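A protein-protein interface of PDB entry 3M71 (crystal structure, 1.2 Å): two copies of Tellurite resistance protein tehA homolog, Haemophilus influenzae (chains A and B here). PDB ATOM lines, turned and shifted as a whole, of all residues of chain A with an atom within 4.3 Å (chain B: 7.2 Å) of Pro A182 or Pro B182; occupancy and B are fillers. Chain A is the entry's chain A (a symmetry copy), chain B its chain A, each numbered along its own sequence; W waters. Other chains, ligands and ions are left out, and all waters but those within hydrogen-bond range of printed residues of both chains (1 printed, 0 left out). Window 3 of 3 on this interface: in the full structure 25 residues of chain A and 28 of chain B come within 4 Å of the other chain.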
ATOM      1  N   ILE A 178      -5.919  34.383  -8.890  1.00  0.00           N
ATOM      2  CA  ILE A 178      -6.669  33.176  -8.566  1.00  0.00           C
ATOM      3  C   ILE A 178      -6.139  32.532  -7.296  1.00  0.00           C
ATOM      4  O   ILE A 178      -6.892  31.877  -6.569  1.00  0.00           O
ATOM      5  CB  ILE A 178      -6.646  32.212  -9.767  1.00  0.00           C
ATOM      6  CG1 ILE A 178      -7.370  32.854 -10.941  1.00  0.00           C
ATOM      7  CG2 ILE A 178      -7.210  30.839  -9.362  1.00  0.00           C
ATOM      8  CD1 ILE A 178      -8.728  33.459 -10.694  1.00  0.00           C
ATOM      9  N   ILE A 179      -4.832  32.687  -7.036  1.00  0.00           N
ATOM     10  CA  ILE A 179      -4.232  32.037  -5.881  1.00  0.00           C
ATOM     11  C   ILE A 179      -4.451  32.884  -4.585  1.00  0.00           C
ATOM     12  O   ILE A 179      -4.484  32.297  -3.510  1.00  0.00           O
ATOM     13  CB  ILE A 179      -2.729  31.818  -6.141  1.00  0.00           C
ATOM     14  CG1 ILE A 179      -2.472  30.829  -7.288  1.00  0.00           C
ATOM     15  CG2 ILE A 179      -1.986  31.350  -4.924  1.00  0.00           C
ATOM     16  CD1 ILE A 179      -3.233  29.656  -7.326  1.00  0.00           C
ATOM     17  N   PHE A 180      -4.641  34.198  -4.692  1.00  0.00           N
ATOM     18  CA  PHE A 180      -4.909  35.041  -3.524  1.00  0.00           C
ATOM     19  C   PHE A 180      -6.392  35.179  -3.179  1.00  0.00           C
ATOM     20  O   PHE A 180      -6.793  35.078  -2.010  1.00  0.00           O
ATOM     21  CB  PHE A 180      -4.289  36.418  -3.651  1.00  0.00           C
ATOM     22  CG  PHE A 180      -4.531  37.287  -2.442  1.00  0.00           C
ATOM     23  CD1 PHE A 180      -3.950  36.951  -1.241  1.00  0.00           C
ATOM     24  CD2 PHE A 180      -5.331  38.394  -2.477  1.00  0.00           C
ATOM     25  CE1 PHE A 180      -4.095  37.722  -0.124  1.00  0.00           C
ATOM     26  CE2 PHE A 180      -5.487  39.207  -1.259  1.00  0.00           C
ATOM     27  CZ  PHE A 180      -4.867  38.760  -0.168  1.00  0.00           C
ATOM     28  N   GLU A 181      -7.244  35.418  -4.182  1.00  0.00           N
ATOM     29  CA  GLU A 181      -8.632  35.688  -3.890  1.00  0.00           C
ATOM     30  C   GLU A 181      -9.330  34.657  -3.015  1.00  0.00           C
ATOM     31  O   GLU A 181     -10.166  35.059  -2.182  1.00  0.00           O
ATOM     32  CB  GLU A 181      -9.437  36.002  -5.170  1.00  0.00           C
ATOM     33  CG  GLU A 181     -10.823  36.482  -4.894  1.00  0.00           C
ATOM     34  CD  GLU A 181     -11.393  37.355  -6.010  1.00  0.00           C
ATOM     35  OE1 GLU A 181     -12.524  37.069  -6.455  1.00  0.00           O
ATOM     36  OE2 GLU A 181     -10.722  38.316  -6.441  1.00  0.00           O
ATOM     37  N   PRO A 182      -9.055  33.345  -3.142  1.00  0.00           N
ATOM     38  CA  PRO A 182      -9.783  32.405  -2.295  1.00  0.00           C
ATOM     39  C   PRO A 182      -9.663  32.733  -0.797  1.00  0.00           C
ATOM     40  O   PRO A 182     -10.663  32.677  -0.057  1.00  0.00           O
ATOM     41  CB  PRO A 182      -9.144  31.050  -2.610  1.00  0.00           C
ATOM     42  CG  PRO A 182      -8.647  31.233  -4.039  1.00  0.00           C
ATOM     43  CD  PRO A 182      -8.168  32.669  -4.085  1.00  0.00           C
ATOM     44  N   VAL A 183      -8.455  33.041  -0.358  1.00  0.00           N
ATOM     45  CA  VAL A 183      -8.233  33.309   1.047  1.00  0.00           C
ATOM     46  C   VAL A 183      -8.707  34.691   1.443  1.00  0.00           C
ATOM     47  O   VAL A 183      -9.140  34.892   2.598  1.00  0.00           O
ATOM     48  CB  VAL A 183      -6.775  33.004   1.483  1.00  0.00           C
ATOM     49  CG1 VAL A 183      -6.442  31.528   1.223  1.00  0.00           C
ATOM     50  CG2 VAL A 183      -5.770  33.935   0.872  1.00  0.00           C
ATOM     51  N   LEU A 184      -8.693  35.652   0.534  1.00  0.00           N
ATOM     52  CA  LEU A 184      -9.272  36.958   0.827  1.00  0.00           C
ATOM     53  C   LEU A 184     -10.769  36.831   1.092  1.00  0.00           C
ATOM     54  O   LEU A 184     -11.263  37.383   2.098  1.00  0.00           O
ATOM     55  CB  LEU A 184      -9.022  37.956  -0.304  1.00  0.00           C
ATOM     56  CG  LEU A 184      -9.666  39.316  -0.103  1.00  0.00           C
ATOM     57  CD1 LEU A 184      -9.097  40.045   1.106  1.00  0.00           C
ATOM     58  CD2 LEU A 184      -9.516  40.160  -1.350  1.00  0.00           C
ATOM     59  N   LEU A 185     -11.533  36.174   0.206  1.00  0.00           N
ATOM     60  CA  LEU A 185     -12.977  36.176   0.394  1.00  0.00           C
ATOM     61  C   LEU A 185     -13.375  35.378   1.636  1.00  0.00           C
ATOM     62  O   LEU A 185     -14.331  35.727   2.328  1.00  0.00           O
ATOM     63  CB  LEU A 185     -13.710  35.703  -0.852  1.00  0.00           C
ATOM     64  CG  LEU A 185     -13.454  36.507  -2.116  1.00  0.00           C
ATOM     65  CD1 LEU A 185     -14.392  36.042  -3.242  1.00  0.00           C
ATOM     66  CD2 LEU A 185     -13.605  38.006  -1.893  1.00  0.00           C
ATOM     67  N   GLN A 186     -12.651  34.296   1.936  1.00  0.00           N
ATOM     68  CA  GLN A 186     -12.924  33.534   3.151  1.00  0.00           C
ATOM     69  C   GLN A 186     -12.683  34.418   4.387  1.00  0.00           C
ATOM     70  O   GLN A 186     -13.467  34.410   5.335  1.00  0.00           O
ATOM     71  CB  GLN A 186     -12.081  32.273   3.208  1.00  0.00           C
ATOM     72  CG  GLN A 186     -12.312  31.388   4.430  1.00  0.00           C
ATOM     73  CD  GLN A 186     -13.567  30.562   4.405  1.00  0.00           C
ATOM     74  OE1 GLN A 186     -14.493  30.788   3.622  1.00  0.00           O
ATOM     75  NE2 GLN A 186     -13.650  29.586   5.331  1.00  0.00           N
ATOM     76  N   THR B 138     -18.241  26.539   6.313  1.00  0.00           N
ATOM     77  CA  THR B 138     -17.621  26.271   5.025  1.00  0.00           C
ATOM     78  C   THR B 138     -18.038  24.886   4.534  1.00  0.00           C
ATOM     79  O   THR B 138     -17.342  23.886   4.739  1.00  0.00           O
ATOM     80  CB  THR B 138     -16.094  26.395   5.132  1.00  0.00           C
ATOM     81  OG1 THR B 138     -15.751  27.609   5.764  1.00  0.00           O
ATOM     82  CG2 THR B 138     -15.452  26.379   3.763  1.00  0.00           C
ATOM     83  N   TYR B 143     -21.671  25.733  -2.928  1.00  0.00           N
ATOM     84  CA  TYR B 143     -21.628  25.642  -4.377  1.00  0.00           C
ATOM     85  C   TYR B 143     -22.962  25.916  -5.065  1.00  0.00           C
ATOM     86  O   TYR B 143     -22.989  26.306  -6.228  1.00  0.00           O
ATOM     87  CB  TYR B 143     -21.173  24.268  -4.849  1.00  0.00           C
ATOM     88  CG  TYR B 143     -19.725  23.876  -4.587  1.00  0.00           C
ATOM     89  CD1 TYR B 143     -18.704  24.657  -4.996  1.00  0.00           C
ATOM     90  CD2 TYR B 143     -19.428  22.681  -3.959  1.00  0.00           C
ATOM     91  CE1 TYR B 143     -17.366  24.281  -4.792  1.00  0.00           C
ATOM     92  CE2 TYR B 143     -18.094  22.308  -3.780  1.00  0.00           C
ATOM     93  CZ  TYR B 143     -17.107  23.094  -4.202  1.00  0.00           C
ATOM     94  OH  TYR B 143     -15.787  22.728  -3.998  1.00  0.00           O
ATOM     95  N   ALA B 176     -15.993  31.580  -9.692  1.00  0.00           N
ATOM     96  CA  ALA B 176     -16.457  31.402  -8.323  1.00  0.00           C
ATOM     97  C   ALA B 176     -16.111  30.019  -7.749  1.00  0.00           C
ATOM     98  O   ALA B 176     -15.810  29.898  -6.557  1.00  0.00           O
ATOM     99  CB  ALA B 176     -17.928  31.641  -8.210  1.00  0.00           C
ATOM    100  N   TRP B 177     -16.176  28.981  -8.584  1.00  0.00           N
ATOM    101  CA  TRP B 177     -15.818  27.636  -8.171  1.00  0.00           C
ATOM    102  C   TRP B 177     -14.371  27.551  -7.719  1.00  0.00           C
ATOM    103  O   TRP B 177     -14.080  27.071  -6.610  1.00  0.00           O
ATOM    104  CB  TRP B 177     -16.087  26.670  -9.337  1.00  0.00           C
ATOM    105  CG  TRP B 177     -15.498  25.311  -9.214  1.00  0.00           C
ATOM    106  CD1 TRP B 177     -15.298  24.583  -8.075  1.00  0.00           C
ATOM    107  CD2 TRP B 177     -14.961  24.540 -10.286  1.00  0.00           C
ATOM    108  NE1 TRP B 177     -14.655  23.405  -8.366  1.00  0.00           N
ATOM    109  CE2 TRP B 177     -14.440  23.340  -9.732  1.00  0.00           C
ATOM    110  CE3 TRP B 177     -14.908  24.705 -11.655  1.00  0.00           C
ATOM    111  CZ2 TRP B 177     -13.840  22.367 -10.511  1.00  0.00           C
ATOM    112  CZ3 TRP B 177     -14.295  23.744 -12.419  1.00  0.00           C
ATOM    113  CH2 TRP B 177     -13.777  22.611 -11.870  1.00  0.00           C
ATOM    114  N   ILE B 178     -13.471  27.971  -8.597  1.00  0.00           N
ATOM    115  CA  ILE B 178     -12.037  27.935  -8.337  1.00  0.00           C
ATOM    116  C   ILE B 178     -11.686  28.758  -7.109  1.00  0.00           C
ATOM    117  O   ILE B 178     -10.710  28.457  -6.415  1.00  0.00           O
ATOM    118  CB  ILE B 178     -11.270  28.394  -9.591  1.00  0.00           C
ATOM    119  CG1 ILE B 178     -11.517  27.407 -10.722  1.00  0.00           C
ATOM    120  CG2 ILE B 178      -9.782  28.604  -9.260  1.00  0.00           C
ATOM    121  CD1 ILE B 178     -11.351  25.938 -10.432  1.00  0.00           C
ATOM    122  N   ILE B 179     -12.462  29.822  -6.850  1.00  0.00           N
ATOM    123  CA  ILE B 179     -12.147  30.704  -5.737  1.00  0.00           C
ATOM    124  C   ILE B 179     -12.710  30.137  -4.394  1.00  0.00           C
ATOM    125  O   ILE B 179     -12.136  30.438  -3.354  1.00  0.00           O
ATOM    126  CB  ILE B 179     -12.720  32.107  -6.019  1.00  0.00           C
ATOM    127  CG1 ILE B 179     -12.046  32.784  -7.222  1.00  0.00           C
ATOM    128  CG2 ILE B 179     -12.631  33.025  -4.836  1.00  0.00           C
ATOM    129  CD1 ILE B 179     -10.652  32.708  -7.321  1.00  0.00           C
ATOM    130  N   PHE B 180     -13.756  29.315  -4.425  1.00  0.00           N
ATOM    131  CA  PHE B 180     -14.297  28.701  -3.209  1.00  0.00           C
ATOM    132  C   PHE B 180     -13.661  27.360  -2.847  1.00  0.00           C
ATOM    133  O   PHE B 180     -13.320  27.103  -1.682  1.00  0.00           O
ATOM    134  CB  PHE B 180     -15.805  28.547  -3.262  1.00  0.00           C
ATOM    135  CG  PHE B 180     -16.381  27.946  -2.004  1.00  0.00           C
ATOM    136  CD1 PHE B 180     -16.325  28.657  -0.828  1.00  0.00           C
ATOM    137  CD2 PHE B 180     -16.939  26.699  -1.971  1.00  0.00           C
ATOM    138  CE1 PHE B 180     -16.868  28.186   0.332  1.00  0.00           C
ATOM    139  CE2 PHE B 180     -17.509  26.201  -0.708  1.00  0.00           C
ATOM    140  CZ  PHE B 180     -17.383  26.998   0.352  1.00  0.00           C
ATOM    141  N   GLU B 181     -13.488  26.468  -3.829  1.00  0.00           N
ATOM    142  CA  GLU B 181     -13.015  25.141  -3.513  1.00  0.00           C
ATOM    143  C   GLU B 181     -11.734  25.082  -2.693  1.00  0.00           C
ATOM    144  O   GLU B 181     -11.625  24.185  -1.833  1.00  0.00           O
ATOM    145  CB  GLU B 181     -12.942  24.244  -4.767  1.00  0.00           C
ATOM    146  CG  GLU B 181     -12.652  22.813  -4.456  1.00  0.00           C
ATOM    147  CD  GLU B 181     -13.174  21.846  -5.516  1.00  0.00           C
ATOM    148  OE1 GLU B 181     -12.381  20.994  -5.970  1.00  0.00           O
ATOM    149  OE2 GLU B 181     -14.360  21.934  -5.897  1.00  0.00           O
ATOM    150  N   PRO B 182     -10.742  25.970  -2.896  1.00  0.00           N
ATOM    151  CA  PRO B 182      -9.526  25.836  -2.099  1.00  0.00           C
ATOM    152  C   PRO B 182      -9.801  25.827  -0.586  1.00  0.00           C
ATOM    153  O   PRO B 182      -9.219  25.015   0.156  1.00  0.00           O
ATOM    154  CB  PRO B 182      -8.689  27.055  -2.495  1.00  0.00           C
ATOM    155  CG  PRO B 182      -9.160  27.345  -3.914  1.00  0.00           C
ATOM    156  CD  PRO B 182     -10.644  27.042  -3.882  1.00  0.00           C
ATOM    157  N   VAL B 183     -10.651  26.736  -0.138  1.00  0.00           N
ATOM    158  CA  VAL B 183     -10.929  26.842   1.278  1.00  0.00           C
ATOM    159  C   VAL B 183     -11.870  25.756   1.755  1.00  0.00           C
ATOM    160  O   VAL B 183     -11.775  25.320   2.923  1.00  0.00           O
ATOM    161  CB  VAL B 183     -11.375  28.272   1.687  1.00  0.00           C
ATOM    162  CG1 VAL B 183     -10.277  29.287   1.341  1.00  0.00           C
ATOM    163  CG2 VAL B 183     -12.710  28.656   1.123  1.00  0.00           C
ATOM    164  N   LEU B 184     -12.750  25.258   0.902  1.00  0.00           N
ATOM    165  CA  LEU B 184     -13.577  24.115   1.273  1.00  0.00           C
ATOM    166  C   LEU B 184     -12.707  22.890   1.540  1.00  0.00           C
ATOM    167  O   LEU B 184     -12.891  22.222   2.579  1.00  0.00           O
ATOM    168  CB  LEU B 184     -14.617  23.795   0.199  1.00  0.00           C
ATOM    169  CG  LEU B 184     -15.463  22.566   0.480  1.00  0.00           C
ATOM    170  CD1 LEU B 184     -16.322  22.736   1.725  1.00  0.00           C
ATOM    171  CD2 LEU B 184     -16.324  22.233  -0.717  1.00  0.00           C
ATOM    172  N   LEU B 185     -11.797  22.527   0.624  1.00  0.00           N
ATOM    173  CA  LEU B 185     -11.069  21.281   0.821  1.00  0.00           C
ATOM    174  C   LEU B 185     -10.123  21.376   2.018  1.00  0.00           C
ATOM    175  O   LEU B 185      -9.915  20.398   2.735  1.00  0.00           O
ATOM    176  CB  LEU B 185     -10.350  20.840  -0.446  1.00  0.00           C
ATOM    177  CG  LEU B 185     -11.232  20.617  -1.663  1.00  0.00           C
ATOM    178  CD1 LEU B 185     -10.413  19.998  -2.808  1.00  0.00           C
ATOM    179  CD2 LEU B 185     -12.443  19.747  -1.355  1.00  0.00           C
ATOM    180  N   GLN B 186      -9.534  22.553   2.251  1.00  0.00           N
ATOM    181  CA  GLN B 186      -8.683  22.739   3.423  1.00  0.00           C
ATOM    182  C   GLN B 186      -9.512  22.548   4.705  1.00  0.00           C
ATOM    183  O   GLN B 186      -9.070  21.906   5.657  1.00  0.00           O
ATOM    184  CB  GLN B 186      -8.012  24.099   3.403  1.00  0.00           C
ATOM    185  CG  GLN B 186      -7.075  24.381   4.574  1.00  0.00           C
ATOM    186  CD  GLN B 186      -5.734  23.706   4.511  1.00  0.00           C
ATOM    187  OE1 GLN B 186      -5.503  22.765   3.748  1.00  0.00           O
ATOM    188  NE2 GLN B 186      -4.806  24.152   5.381  1.00  0.00           N
ATOM    189  N   HIS B 187     -10.727  23.098   4.719  1.00  0.00           N
ATOM    190  CA  HIS B 187     -11.637  22.931   5.855  1.00  0.00           C
ATOM    191  C   HIS B 187     -11.971  21.465   6.079  1.00  0.00           C
ATOM    192  O   HIS B 187     -11.959  20.988   7.227  1.00  0.00           O
ATOM    193  CB  HIS B 187     -12.906  23.727   5.646  1.00  0.00           C
ATOM    194  CG  HIS B 187     -13.885  23.589   6.761  1.00  0.00           C
ATOM    195  ND1 HIS B 187     -13.609  24.050   8.028  1.00  0.00           N
ATOM    196  CD2 HIS B 187     -15.110  23.033   6.787  1.00  0.00           C
ATOM    197  CE1 HIS B 187     -14.656  23.776   8.791  1.00  0.00           C
ATOM    198  NE2 HIS B 187     -15.572  23.151   8.067  1.00  0.00           N
ATOM    199  N   LEU B 188     -12.301  20.738   5.014  1.00  0.00           N
ATOM    200  CA  LEU B 188     -12.636  19.324   5.170  1.00  0.00           C
ATOM    201  C   LEU B 188     -11.448  18.543   5.701  1.00  0.00           C
ATOM    202  O   LEU B 188     -11.600  17.607   6.497  1.00  0.00           O
ATOM    203  CB  LEU B 188     -13.138  18.731   3.860  1.00  0.00           C
ATOM    204  CG  LEU B 188     -14.434  19.309   3.314  1.00  0.00           C
ATOM    205  CD1 LEU B 188     -14.703  18.647   1.958  1.00  0.00           C
ATOM    206  CD2 LEU B 188     -15.576  19.096   4.271  1.00  0.00           C
ATOM    207  N   ARG B 189     -10.235  18.871   5.245  1.00  0.00           N
ATOM    208  CA  ARG B 189      -9.047  18.187   5.749  1.00  0.00           C
ATOM    209  C   ARG B 189      -8.876  18.369   7.248  1.00  0.00           C
ATOM    210  O   ARG B 189      -8.473  17.422   7.942  1.00  0.00           O
ATOM    211  CB  ARG B 189      -7.759  18.672   5.050  1.00  0.00           C
ATOM    212  CG  ARG B 189      -7.542  18.156   3.628  1.00  0.00           C
ATOM    213  CD  ARG B 189      -6.142  18.475   3.122  1.00  0.00           C
ATOM    214  NE  ARG B 189      -5.980  19.892   2.708  1.00  0.00           N
ATOM    215  CZ  ARG B 189      -6.264  20.345   1.505  1.00  0.00           C
ATOM    216  NH1 ARG B 189      -6.648  19.518   0.552  1.00  0.00           N
ATOM    217  NH2 ARG B 189      -6.082  21.623   1.238  1.00  0.00           N
HETATM  218  O   HOH W   1     -13.136  31.814  -1.142  1.00  0.00           O
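OG1 of Thr B138 lies within hydrogen-bond range of NE2 of Gln A186.
Among the printed residues, pairs that only touch across the chains: Pro A182 with Ile B179 (3.1 Å), Ile A178 with Ile B178 (3.4 Å), Pro A182 with Val B183 (3.7 Å), Gln A186 with Val B183 (3.7 Å), Leu A185 with Ile B179 (3.8 Å), Glu A181 with Ile B179 (3.9 Å), Ile A178 with Ile B179 (3.9 Å) and Pro A182 with Pro B182 (3.9 Å).
Of chain A, only Pro A182 comes within 4 Å of Pro B182. Of the printed residues of chain B, Leu A185 touches Ile B179. Of the printed residues of chain B, Ile A178 touches Ile B178 (3.4 Å) and Ile B179 (3.9 Å). Printed residues of chain B within 4 Å of Gln A186: Thr B138 (2.9 Å) and Val B183 (3.7 Å). Printed residues of chain A within 4 Å of Val B183: Pro A182 (3.7 Å) and Gln A186 (3.7 Å). Printed residues of chain B within 4 Å of Glu A181: Ile B179. Leu B184 touches none of the printed residues of chain A. The nearest printed residue of chain A that does not touch Ile B178 is Pro A182 (4.2 Å).
Of the 9 printed residues of chain A, 5 touch a printed residue of chain B. Hydrophobic or aromatic side chains of chain A that line the printed part of chain B: Ile A178, Pro A182 and Leu A185. Among the printed residues, no Asp or Glu carboxylate lies within 4 Å of a Lys or Arg side-chain nitrogen of the other chain.
Pro A182 touches Ile B179, but with the chains exchanged Ile A179 does not touch Pro B182 (6.8 Å). Pro A182 touches its own counterpart, Pro B182. Pro A182 touches Val B183, but with the chains exchanged Val A183 does not touch Pro B182 (6.2 Å). Gln A186 touches Val B183, but with the chains exchanged Val A183 does not touch Gln B186 (7.9 Å).
Water W1 bridges the backbone carbonyl oxygen (O) of Ile B179 (2.8 Å) and the backbone carbonyl oxygen (O) of Pro A182 (2.8 Å).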
